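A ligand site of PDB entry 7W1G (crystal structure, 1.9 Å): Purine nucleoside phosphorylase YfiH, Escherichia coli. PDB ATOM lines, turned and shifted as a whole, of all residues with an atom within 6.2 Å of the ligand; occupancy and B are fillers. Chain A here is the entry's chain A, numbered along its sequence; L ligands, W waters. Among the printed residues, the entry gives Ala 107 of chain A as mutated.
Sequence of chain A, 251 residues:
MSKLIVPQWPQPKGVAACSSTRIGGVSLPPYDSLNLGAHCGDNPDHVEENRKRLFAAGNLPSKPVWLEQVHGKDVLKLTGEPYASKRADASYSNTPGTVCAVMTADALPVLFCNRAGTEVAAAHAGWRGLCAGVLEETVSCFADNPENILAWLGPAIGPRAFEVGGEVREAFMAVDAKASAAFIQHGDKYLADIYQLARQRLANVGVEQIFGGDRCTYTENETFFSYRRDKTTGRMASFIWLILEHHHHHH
OD2 of Asp 106 lies within hydrogen-bond range of N of Tyr 227 (3.3 Å). The backbone NH of Tyr 227 sits at hydrogen-bond distance from the backbone carbonyl oxygen of Ala 105 (2.8 Å). The guanidinium group (NH1) of Arg 228 sits at hydrogen-bond distance from the backbone carbonyl oxygen (O) of Glu 163. The side-chain carboxylate (OD2) of Asp 106 lies within hydrogen-bond range of the backbone NH (N) of Arg 228, 2.7 Å away. The backbone NH of Val 164 lies within hydrogen-bond range of the backbone carbonyl oxygen of Tyr 190 (2.8 Å). N of Ile 157 is in hydrogen-bond range of O of Asp 106 (2.8 Å).
O7 of the ligand sits at hydrogen-bond distance from NE1 of Trp 127 (3.0 Å). NE of Arg 228 lies within salt-bridge range of O11 of the ligand. NE2 of His 124 sits at hydrogen-bond distance from O9 of the ligand, at 2.8 Å. The backbone NH (N) of Gly 165 lies within hydrogen-bond range of an oxygen (O16) of the ligand (2.7 Å). OE1 of Glu 167 is in hydrogen-bond range of O16 of the ligand, 2.5 Å away. N of Ala 107 is in hydrogen-bond range of O13 of the ligand (2.9 Å). An oxygen (O13) of the ligand lies within hydrogen-bond range of the backbone NH (N) of Asp 106. N of Ala 105 sits at hydrogen-bond distance from O13 of the ligand. The guanidinium group (NH2) of Arg 128 is in salt-bridge range of an oxygen (O7) of the ligand.
An oxygen (O17) of the ligand lies close to the backbone carbonyl oxygen of Glu 163. Merely in contact with the ligand: Lys 189 (3.0 Å), Gly 126 (3.2 Å), His 71 (3.3 Å), Val 164 (3.3 Å), Thr 104 (3.4 Å), Tyr 227 (3.4 Å), Val 168 (3.7 Å) and Phe 162 (3.8 Å). Of the 27 residues printed, 18 come within 4 Å of the ligand. The nearest printed residue that does not touch the ligand is Ile 157 (4.01 Å).
Water W2 lies within hydrogen-bond range of an oxygen (O9) of the ligand (2.5 Å), the backbone carbonyl oxygen (O) of Met 103 (2.8 Å) and a ring nitrogen (NE2) of His 124 (3.4 Å). Water W1 lies within hydrogen-bond range of a nitrogen (N1) of the ligand (2.6 Å) and the side-chain carboxylate of Asp 106 (2.9 Å). Water W3 bridges O11 of the ligand and NE of Arg 228. Water W4 lies within hydrogen-bond range of ND1 of His 71 (2.9 Å), NH1 of Arg 128 (2.9 Å) and N of Trp 127 (3.5 Å).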
ATOM      1  N   GLN A  69      -4.969   5.459  -9.276  1.00  0.00           N
ATOM      2  CA  GLN A  69      -3.720   4.723  -9.585  1.00  0.00           C
ATOM      3  C   GLN A  69      -3.623   4.653 -11.113  1.00  0.00           C
ATOM      4  O   GLN A  69      -4.610   4.280 -11.733  1.00  0.00           O
ATOM      5  CB  GLN A  69      -3.707   3.333  -8.919  1.00  0.00           C
ATOM      6  CG  GLN A  69      -3.750   3.383  -7.379  1.00  0.00           C
ATOM      7  CD  GLN A  69      -3.853   2.055  -6.667  1.00  0.00           C
ATOM      8  OE1 GLN A  69      -3.939   2.001  -5.430  1.00  0.00           O
ATOM      9  NE2 GLN A  69      -3.814   0.965  -7.420  1.00  0.00           N
ATOM     10  N   HIS A  71      -0.623   3.302 -12.673  1.00  0.00           N
ATOM     11  CA  HIS A  71       0.572   2.454 -12.876  1.00  0.00           C
ATOM     12  C   HIS A  71       1.806   3.329 -13.173  1.00  0.00           C
ATOM     13  O   HIS A  71       2.645   2.882 -13.951  1.00  0.00           O
ATOM     14  CB  HIS A  71       0.308   1.426 -13.965  1.00  0.00           C
ATOM     15  CG  HIS A  71      -0.598   0.319 -13.516  1.00  0.00           C
ATOM     16  ND1 HIS A  71      -0.106  -0.878 -13.023  1.00  0.00           N
ATOM     17  CD2 HIS A  71      -1.948   0.246 -13.441  1.00  0.00           C
ATOM     18  CE1 HIS A  71      -1.121  -1.656 -12.689  1.00  0.00           C
ATOM     19  NE2 HIS A  71      -2.260  -0.992 -12.935  1.00  0.00           N
ATOM     20  N   MET A 103      -4.316  -0.416  -3.947  1.00  0.00           N
ATOM     21  CA  MET A 103      -5.326  -1.364  -4.458  1.00  0.00           C
ATOM     22  C   MET A 103      -4.635  -2.306  -5.449  1.00  0.00           C
ATOM     23  O   MET A 103      -3.962  -1.789  -6.365  1.00  0.00           O
ATOM     24  CB  MET A 103      -6.424  -0.575  -5.165  1.00  0.00           C
ATOM     25  CG  MET A 103      -7.618  -1.404  -5.474  1.00  0.00           C
ATOM     26  SD  MET A 103      -8.795  -1.285  -4.147  1.00  0.00           S
ATOM     27  CE  MET A 103      -9.325   0.398  -4.448  1.00  0.00           C
ATOM     28  N   THR A 104      -4.762  -3.633  -5.281  1.00  0.00           N
ATOM     29  CA  THR A 104      -4.055  -4.630  -6.134  1.00  0.00           C
ATOM     30  C   THR A 104      -4.869  -5.905  -6.358  1.00  0.00           C
ATOM     31  O   THR A 104      -5.755  -6.237  -5.522  1.00  0.00           O
ATOM     32  CB  THR A 104      -2.726  -5.107  -5.524  1.00  0.00           C
ATOM     33  OG1 THR A 104      -2.972  -5.936  -4.390  1.00  0.00           O
ATOM     34  CG2 THR A 104      -1.773  -4.001  -5.096  1.00  0.00           C
ATOM     35  N   ALA A 105      -4.496  -6.632  -7.422  1.00  0.00           N
ATOM     36  CA  ALA A 105      -4.949  -8.014  -7.729  1.00  0.00           C
ATOM     37  C   ALA A 105      -3.924  -8.646  -8.684  1.00  0.00           C
ATOM     38  O   ALA A 105      -4.284  -9.074  -9.805  1.00  0.00           O
ATOM     39  CB  ALA A 105      -6.337  -8.025  -8.274  1.00  0.00           C
ATOM     40  N   ASP A 106      -2.660  -8.594  -8.252  1.00  0.00           N
ATOM     41  CA  ASP A 106      -1.458  -9.223  -8.854  1.00  0.00           C
ATOM     42  C   ASP A 106      -0.289  -8.257  -8.695  1.00  0.00           C
ATOM     43  O   ASP A 106       0.813  -8.733  -8.430  1.00  0.00           O
ATOM     44  CB  ASP A 106      -1.557  -9.554 -10.346  1.00  0.00           C
ATOM     45  CG  ASP A 106      -2.382 -10.797 -10.702  1.00  0.00           C
ATOM     46  OD1 ASP A 106      -2.647 -11.656  -9.830  1.00  0.00           O
ATOM     47  OD2 ASP A 106      -2.758 -10.873 -11.863  1.00  0.00           O
ATOM     48  N   ALA A 107      -0.536  -6.957  -8.839  1.00  0.00           N
ATOM     49  CA  ALA A 107       0.510  -5.929  -8.611  1.00  0.00           C
ATOM     50  C   ALA A 107       1.084  -6.107  -7.201  1.00  0.00           C
ATOM     51  O   ALA A 107       0.358  -6.489  -6.276  1.00  0.00           O
ATOM     52  CB  ALA A 107      -0.043  -4.524  -8.831  1.00  0.00           C
ATOM     53  N   LEU A 108       2.381  -5.850  -7.029  1.00  0.00           N
ATOM     54  CA  LEU A 108       3.015  -5.860  -5.700  1.00  0.00           C
ATOM     55  C   LEU A 108       2.626  -4.614  -4.885  1.00  0.00           C
ATOM     56  O   LEU A 108       2.960  -3.483  -5.270  1.00  0.00           O
ATOM     57  CB  LEU A 108       4.524  -5.901  -5.925  1.00  0.00           C
ATOM     58  CG  LEU A 108       5.380  -5.880  -4.661  1.00  0.00           C
ATOM     59  CD1 LEU A 108       5.201  -7.156  -3.833  1.00  0.00           C
ATOM     60  CD2 LEU A 108       6.837  -5.669  -5.027  1.00  0.00           C
ATOM     61  N   HIS A 124       1.848   1.030  -4.853  1.00  0.00           N
ATOM     62  CA  HIS A 124       1.307   0.120  -5.887  1.00  0.00           C
ATOM     63  C   HIS A 124       2.386  -0.125  -6.946  1.00  0.00           C
ATOM     64  O   HIS A 124       2.654   0.777  -7.751  1.00  0.00           O
ATOM     65  CB  HIS A 124       0.028   0.745  -6.449  1.00  0.00           C
ATOM     66  CG  HIS A 124      -0.520   0.076  -7.663  1.00  0.00           C
ATOM     67  ND1 HIS A 124      -0.584   0.721  -8.883  1.00  0.00           N
ATOM     68  CD2 HIS A 124      -1.053  -1.152  -7.844  1.00  0.00           C
ATOM     69  CE1 HIS A 124      -1.139  -0.086  -9.766  1.00  0.00           C
ATOM     70  NE2 HIS A 124      -1.427  -1.243  -9.155  1.00  0.00           N
ATOM     71  N   ALA A 125       2.981  -1.320  -6.946  1.00  0.00           N
ATOM     72  CA  ALA A 125       4.077  -1.678  -7.871  1.00  0.00           C
ATOM     73  C   ALA A 125       3.619  -2.831  -8.764  1.00  0.00           C
ATOM     74  O   ALA A 125       4.114  -3.969  -8.628  1.00  0.00           O
ATOM     75  CB  ALA A 125       5.351  -1.992  -7.111  1.00  0.00           C
ATOM     76  N   GLY A 126       2.740  -2.517  -9.704  1.00  0.00           N
ATOM     77  CA  GLY A 126       2.617  -3.321 -10.940  1.00  0.00           C
ATOM     78  C   GLY A 126       3.913  -3.239 -11.729  1.00  0.00           C
ATOM     79  O   GLY A 126       4.763  -2.393 -11.404  1.00  0.00           O
ATOM     80  N   TRP A 127       4.140  -4.116 -12.700  1.00  0.00           N
ATOM     81  CA  TRP A 127       5.426  -4.111 -13.449  1.00  0.00           C
ATOM     82  C   TRP A 127       5.727  -2.725 -14.035  1.00  0.00           C
ATOM     83  O   TRP A 127       6.913  -2.284 -13.978  1.00  0.00           O
ATOM     84  CB  TRP A 127       5.469  -5.221 -14.493  1.00  0.00           C
ATOM     85  CG  TRP A 127       4.546  -5.084 -15.656  1.00  0.00           C
ATOM     86  CD1 TRP A 127       3.324  -5.668 -15.829  1.00  0.00           C
ATOM     87  CD2 TRP A 127       4.828  -4.385 -16.887  1.00  0.00           C
ATOM     88  NE1 TRP A 127       2.833  -5.379 -17.078  1.00  0.00           N
ATOM     89  CE2 TRP A 127       3.717  -4.584 -17.737  1.00  0.00           C
ATOM     90  CE3 TRP A 127       5.901  -3.619 -17.349  1.00  0.00           C
ATOM     91  CZ2 TRP A 127       3.634  -4.008 -19.009  1.00  0.00           C
ATOM     92  CZ3 TRP A 127       5.816  -3.049 -18.601  1.00  0.00           C
ATOM     93  CH2 TRP A 127       4.702  -3.248 -19.417  1.00  0.00           C
ATOM     94  N   ARG A 128       4.711  -2.021 -14.533  1.00  0.00           N
ATOM     95  CA  ARG A 128       4.932  -0.697 -15.192  1.00  0.00           C
ATOM     96  C   ARG A 128       5.541   0.270 -14.176  1.00  0.00           C
ATOM     97  O   ARG A 128       6.615   0.833 -14.475  1.00  0.00           O
ATOM     98  CB  ARG A 128       3.638  -0.170 -15.820  1.00  0.00           C
ATOM     99  CG  ARG A 128       3.254  -0.917 -17.087  1.00  0.00           C
ATOM    100  CD  ARG A 128       1.983  -0.374 -17.722  1.00  0.00           C
ATOM    101  NE  ARG A 128       1.507  -1.283 -18.747  1.00  0.00           N
ATOM    102  CZ  ARG A 128       0.803  -2.368 -18.495  1.00  0.00           C
ATOM    103  NH1 ARG A 128       0.538  -2.680 -17.237  1.00  0.00           N
ATOM    104  NH2 ARG A 128       0.399  -3.149 -19.482  1.00  0.00           N
ATOM    105  N   ILE A 157       1.602 -11.379  -7.759  1.00  0.00           N
ATOM    106  CA  ILE A 157       1.660 -12.545  -8.663  1.00  0.00           C
ATOM    107  C   ILE A 157       3.096 -13.078  -8.628  1.00  0.00           C
ATOM    108  O   ILE A 157       4.014 -12.336  -9.037  1.00  0.00           O
ATOM    109  CB  ILE A 157       1.121 -12.236 -10.075  1.00  0.00           C
ATOM    110  CG1 ILE A 157       1.158 -13.521 -10.907  1.00  0.00           C
ATOM    111  CG2 ILE A 157       1.840 -11.073 -10.730  1.00  0.00           C
ATOM    112  CD1 ILE A 157       0.145 -13.544 -12.032  1.00  0.00           C
ATOM    113  N   PHE A 162       3.757 -15.511 -13.156  1.00  0.00           N
ATOM    114  CA  PHE A 162       3.850 -14.181 -13.811  1.00  0.00           C
ATOM    115  C   PHE A 162       4.624 -14.313 -15.136  1.00  0.00           C
ATOM    116  O   PHE A 162       5.765 -13.810 -15.261  1.00  0.00           O
ATOM    117  CB  PHE A 162       4.399 -13.142 -12.833  1.00  0.00           C
ATOM    118  CG  PHE A 162       4.373 -11.707 -13.310  1.00  0.00           C
ATOM    119  CD1 PHE A 162       3.393 -11.232 -14.180  1.00  0.00           C
ATOM    120  CD2 PHE A 162       5.369 -10.835 -12.896  1.00  0.00           C
ATOM    121  CE1 PHE A 162       3.400  -9.914 -14.604  1.00  0.00           C
ATOM    122  CE2 PHE A 162       5.363  -9.513 -13.315  1.00  0.00           C
ATOM    123  CZ  PHE A 162       4.379  -9.045 -14.174  1.00  0.00           C
ATOM    124  N   GLU A 163       3.934 -14.879 -16.131  1.00  0.00           N
ATOM    125  CA  GLU A 163       4.384 -14.976 -17.542  1.00  0.00           C
ATOM    126  C   GLU A 163       4.329 -13.592 -18.193  1.00  0.00           C
ATOM    127  O   GLU A 163       3.241 -12.969 -18.195  1.00  0.00           O
ATOM    128  CB  GLU A 163       3.496 -15.949 -18.332  1.00  0.00           C
ATOM    129  CG  GLU A 163       4.015 -16.264 -19.720  1.00  0.00           C
ATOM    130  CD  GLU A 163       3.690 -17.652 -20.285  1.00  0.00           C
ATOM    131  OE1 GLU A 163       4.076 -17.910 -21.442  1.00  0.00           O
ATOM    132  OE2 GLU A 163       3.075 -18.484 -19.565  1.00  0.00           O
ATOM    133  N   VAL A 164       5.457 -13.119 -18.731  1.00  0.00           N
ATOM    134  CA  VAL A 164       5.540 -11.816 -19.438  1.00  0.00           C
ATOM    135  C   VAL A 164       6.280 -12.028 -20.768  1.00  0.00           C
ATOM    136  O   VAL A 164       7.100 -12.968 -20.847  1.00  0.00           O
ATOM    137  CB  VAL A 164       6.228 -10.778 -18.540  1.00  0.00           C
ATOM    138  CG1 VAL A 164       5.476 -10.621 -17.211  1.00  0.00           C
ATOM    139  CG2 VAL A 164       7.682 -11.142 -18.305  1.00  0.00           C
ATOM    140  N   GLY A 165       5.987 -11.204 -21.755  1.00  0.00           N
ATOM    141  CA  GLY A 165       6.721 -11.133 -23.038  1.00  0.00           C
ATOM    142  C   GLY A 165       8.036 -10.388 -22.853  1.00  0.00           C
ATOM    143  O   GLY A 165       8.215  -9.760 -21.800  1.00  0.00           O
ATOM    144  N   GLY A 166       8.926 -10.439 -23.850  1.00  0.00           N
ATOM    145  CA  GLY A 166      10.259  -9.791 -23.829  1.00  0.00           C
ATOM    146  C   GLY A 166      10.156  -8.278 -23.708  1.00  0.00           C
ATOM    147  O   GLY A 166      11.167  -7.648 -23.341  1.00  0.00           O
ATOM    148  N   GLU A 167       8.989  -7.708 -23.974  1.00  0.00           N
ATOM    149  CA  GLU A 167       8.709  -6.250 -23.903  1.00  0.00           C
ATOM    150  C   GLU A 167       8.968  -5.780 -22.477  1.00  0.00           C
ATOM    151  O   GLU A 167       9.691  -4.782 -22.275  1.00  0.00           O
ATOM    152  CB  GLU A 167       7.250  -5.920 -24.235  1.00  0.00           C
ATOM    153  CG  GLU A 167       6.562  -6.878 -25.200  1.00  0.00           C
ATOM    154  CD  GLU A 167       5.330  -7.595 -24.657  1.00  0.00           C
ATOM    155  OE1 GLU A 167       4.689  -7.062 -23.728  1.00  0.00           O
ATOM    156  OE2 GLU A 167       4.997  -8.677 -25.215  1.00  0.00           O
ATOM    157  N   VAL A 168       8.376  -6.489 -21.520  1.00  0.00           N
ATOM    158  CA  VAL A 168       8.518  -6.182 -20.066  1.00  0.00           C
ATOM    159  C   VAL A 168       9.983  -6.376 -19.651  1.00  0.00           C
ATOM    160  O   VAL A 168      10.471  -5.511 -18.900  1.00  0.00           O
ATOM    161  CB  VAL A 168       7.566  -7.028 -19.207  1.00  0.00           C
ATOM    162  CG1 VAL A 168       7.706  -6.670 -17.728  1.00  0.00           C
ATOM    163  CG2 VAL A 168       6.121  -6.867 -19.633  1.00  0.00           C
ATOM    164  N   LYS A 189       8.063 -17.069 -23.867  1.00  0.00           N
ATOM    165  CA  LYS A 189       7.904 -15.940 -22.920  1.00  0.00           C
ATOM    166  C   LYS A 189       8.893 -16.121 -21.761  1.00  0.00           C
ATOM    167  O   LYS A 189       9.815 -16.968 -21.869  1.00  0.00           O
ATOM    168  CB  LYS A 189       6.459 -15.901 -22.441  1.00  0.00           C
ATOM    169  CG  LYS A 189       5.428 -16.087 -23.540  1.00  0.00           C
ATOM    170  CD  LYS A 189       4.147 -15.337 -23.304  1.00  0.00           C
ATOM    171  CE  LYS A 189       3.587 -14.757 -24.579  1.00  0.00           C
ATOM    172  NZ  LYS A 189       4.515 -13.762 -25.173  1.00  0.00           N
ATOM    173  N   TYR A 190       8.725 -15.316 -20.710  1.00  0.00           N
ATOM    174  CA  TYR A 190       9.564 -15.342 -19.487  1.00  0.00           C
ATOM    175  C   TYR A 190       8.625 -15.426 -18.292  1.00  0.00           C
ATOM    176  O   TYR A 190       7.484 -14.964 -18.385  1.00  0.00           O
ATOM    177  CB  TYR A 190      10.483 -14.125 -19.464  1.00  0.00           C
ATOM    178  CG  TYR A 190      11.224 -13.961 -20.762  1.00  0.00           C
ATOM    179  CD1 TYR A 190      10.593 -13.410 -21.877  1.00  0.00           C
ATOM    180  CD2 TYR A 190      12.521 -14.404 -20.904  1.00  0.00           C
ATOM    181  CE1 TYR A 190      11.261 -13.303 -23.091  1.00  0.00           C
ATOM    182  CE2 TYR A 190      13.191 -14.319 -22.121  1.00  0.00           C
ATOM    183  CZ  TYR A 190      12.554 -13.767 -23.212  1.00  0.00           C
ATOM    184  OH  TYR A 190      13.203 -13.663 -24.410  1.00  0.00           O
ATOM    185  N   ILE A 194       8.630 -10.762  -9.484  1.00  0.00           N
ATOM    186  CA  ILE A 194       8.311  -9.370  -9.065  1.00  0.00           C
ATOM    187  C   ILE A 194       8.951  -9.092  -7.682  1.00  0.00           C
ATOM    188  O   ILE A 194       9.438  -7.969  -7.483  1.00  0.00           O
ATOM    189  CB  ILE A 194       6.785  -9.136  -9.084  1.00  0.00           C
ATOM    190  CG1 ILE A 194       6.457  -7.644  -9.184  1.00  0.00           C
ATOM    191  CG2 ILE A 194       6.110  -9.806  -7.892  1.00  0.00           C
ATOM    192  CD1 ILE A 194       5.020  -7.384  -9.604  1.00  0.00           C
ATOM    193  N   TYR A 227      -5.981 -10.660 -11.425  1.00  0.00           N
ATOM    194  CA  TYR A 227      -6.320 -10.201 -12.778  1.00  0.00           C
ATOM    195  C   TYR A 227      -5.838 -11.256 -13.769  1.00  0.00           C
ATOM    196  O   TYR A 227      -6.645 -11.674 -14.647  1.00  0.00           O
ATOM    197  CB  TYR A 227      -5.742  -8.820 -13.025  1.00  0.00           C
ATOM    198  CG  TYR A 227      -5.806  -8.435 -14.469  1.00  0.00           C
ATOM    199  CD1 TYR A 227      -7.025  -8.337 -15.118  1.00  0.00           C
ATOM    200  CD2 TYR A 227      -4.661  -8.218 -15.204  1.00  0.00           C
ATOM    201  CE1 TYR A 227      -7.096  -8.030 -16.470  1.00  0.00           C
ATOM    202  CE2 TYR A 227      -4.720  -7.871 -16.547  1.00  0.00           C
ATOM    203  CZ  TYR A 227      -5.943  -7.779 -17.184  1.00  0.00           C
ATOM    204  OH  TYR A 227      -6.057  -7.449 -18.498  1.00  0.00           O
ATOM    205  N   ARG A 228      -4.589 -11.712 -13.639  1.00  0.00           N
ATOM    206  CA  ARG A 228      -4.041 -12.761 -14.557  1.00  0.00           C
ATOM    207  C   ARG A 228      -4.943 -13.996 -14.567  1.00  0.00           C
ATOM    208  O   ARG A 228      -5.342 -14.408 -15.652  1.00  0.00           O
ATOM    209  CB  ARG A 228      -2.629 -13.211 -14.198  1.00  0.00           C
ATOM    210  CG  ARG A 228      -1.989 -14.090 -15.261  1.00  0.00           C
ATOM    211  CD  ARG A 228      -1.912 -13.447 -16.638  1.00  0.00           C
ATOM    212  NE  ARG A 228      -0.996 -12.323 -16.717  1.00  0.00           N
ATOM    213  CZ  ARG A 228       0.298 -12.388 -17.049  1.00  0.00           C
ATOM    214  NH1 ARG A 228       0.867 -13.546 -17.346  1.00  0.00           N
ATOM    215  NH2 ARG A 228       1.002 -11.275 -17.108  1.00  0.00           N
ATOM    216  N   ARG A 235     -10.577  -6.504  -6.339  1.00  0.00           N
ATOM    217  CA  ARG A 235      -9.289  -5.907  -5.912  1.00  0.00           C
ATOM    218  C   ARG A 235      -9.200  -6.045  -4.402  1.00  0.00           C
ATOM    219  O   ARG A 235     -10.246  -5.899  -3.715  1.00  0.00           O
ATOM    220  CB  ARG A 235      -9.148  -4.458  -6.340  1.00  0.00           C
ATOM    221  CG  ARG A 235      -9.291  -4.222  -7.844  1.00  0.00           C
ATOM    222  CD  ARG A 235      -8.045  -4.541  -8.637  1.00  0.00           C
ATOM    223  NE  ARG A 235      -8.239  -4.186 -10.039  1.00  0.00           N
ATOM    224  CZ  ARG A 235      -8.872  -4.924 -10.941  1.00  0.00           C
ATOM    225  NH1 ARG A 235      -9.386  -6.095 -10.625  1.00  0.00           N
ATOM    226  NH2 ARG A 235      -8.998  -4.469 -12.177  1.00  0.00           N
HETATM  227  C1  LIG L   1      -0.856  -5.670 -15.711  1.00  0.00           C
HETATM  228  O1  LIG L   1      -1.472  -6.894 -16.033  1.00  0.00           O
HETATM  229  C2  LIG L   1      -1.068  -5.409 -14.211  1.00  0.00           C
HETATM  230  N1  LIG L   1      -0.513  -6.506 -13.435  1.00  0.00           N
HETATM  231  C3  LIG L   1      -2.534  -5.096 -13.926  1.00  0.00           C
HETATM  232  O2  LIG L   1      -2.607  -4.552 -12.611  1.00  0.00           O
HETATM  233  C4  LIG L   1      -3.055  -4.020 -14.886  1.00  0.00           C
HETATM  234  O3  LIG L   1      -4.448  -3.794 -14.729  1.00  0.00           O
HETATM  235  C5  LIG L   1      -2.810  -4.448 -16.326  1.00  0.00           C
HETATM  236  O4  LIG L   1      -1.400  -4.641 -16.519  1.00  0.00           O
HETATM  237  C6  LIG L   1      -3.221  -3.381 -17.316  1.00  0.00           C
HETATM  238  O5  LIG L   1      -2.983  -3.860 -18.598  1.00  0.00           O
HETATM  239  C7  LIG L   1       0.693  -6.506 -12.859  1.00  0.00           C
HETATM  240  O6  LIG L   1       1.071  -7.369 -12.054  1.00  0.00           O
HETATM  241  C8  LIG L   1       1.569  -5.365 -13.199  1.00  0.00           C
HETATM  242  P1  LIG L   1      -0.288  -6.966 -19.431  1.00  0.00           P
HETATM  243  P2  LIG L   1      -0.701  -8.102 -16.734  1.00  0.00           P
HETATM  244  O7  LIG L   1       0.336  -5.790 -18.766  1.00  0.00           O
HETATM  245  O8  LIG L   1       0.767  -7.999 -16.465  1.00  0.00           O
HETATM  246  C9  LIG L   1       2.398 -10.891 -21.053  1.00  0.00           C
HETATM  247  C10 LIG L   1      -2.945  -4.703 -10.251  1.00  0.00           C
HETATM  248  O9  LIG L   1      -2.818  -3.457 -10.266  1.00  0.00           O
HETATM  249  N2  LIG L   1       1.316 -11.849 -20.817  1.00  0.00           N
HETATM  250  O10 LIG L   1      -1.245  -6.720 -20.542  1.00  0.00           O
HETATM  251  O11 LIG L   1      -1.433  -9.348 -16.358  1.00  0.00           O
HETATM  252  C11 LIG L   1       2.041  -9.799 -22.059  1.00  0.00           C
HETATM  253  O12 LIG L   1       2.181 -10.336 -23.344  1.00  0.00           O
HETATM  254  C12 LIG L   1      -3.160  -5.378 -11.582  1.00  0.00           C
HETATM  255  O13 LIG L   1      -2.906  -5.413  -9.228  1.00  0.00           O
HETATM  256  C13 LIG L   1       1.595 -13.183 -21.026  1.00  0.00           C
HETATM  257  O14 LIG L   1       2.686 -13.609 -21.403  1.00  0.00           O
HETATM  258  O15 LIG L   1      -1.000  -7.845 -18.298  1.00  0.00           O
HETATM  259  C14 LIG L   1       3.083  -8.749 -21.668  1.00  0.00           C
HETATM  260  O16 LIG L   1       4.357  -9.070 -22.195  1.00  0.00           O
HETATM  261  C15 LIG L   1      -4.634  -5.553 -11.823  1.00  0.00           C
HETATM  262  N3  LIG L   1       0.548 -14.026 -20.782  1.00  0.00           N
HETATM  263  C16 LIG L   1       3.086  -8.861 -20.137  1.00  0.00           C
HETATM  264  O17 LIG L   1       2.684 -10.230 -19.855  1.00  0.00           O
HETATM  265  C17 LIG L   1      -0.711 -13.680 -20.354  1.00  0.00           C
HETATM  266  O18 LIG L   1      -1.540 -14.570 -20.158  1.00  0.00           O
HETATM  267  C18 LIG L   1       2.179  -7.914 -19.399  1.00  0.00           C
HETATM  268  O19 LIG L   1       0.839  -8.000 -19.956  1.00  0.00           O
HETATM  269  C19 LIG L   1      -0.933 -12.271 -20.158  1.00  0.00           C
HETATM  270  C20 LIG L   1       0.083 -11.414 -20.390  1.00  0.00           C
HETATM  271  O   HOH W   1      -1.623  -8.881 -13.669  1.00  0.00           O
HETATM  272  O   HOH W   2      -4.608  -2.369  -8.983  1.00  0.00           O
HETATM  273  O   HOH W   3      -3.293 -10.151 -18.153  1.00  0.00           O
HETATM  274  O   HOH W   4       1.678  -2.499 -14.550  1.00  0.00           O
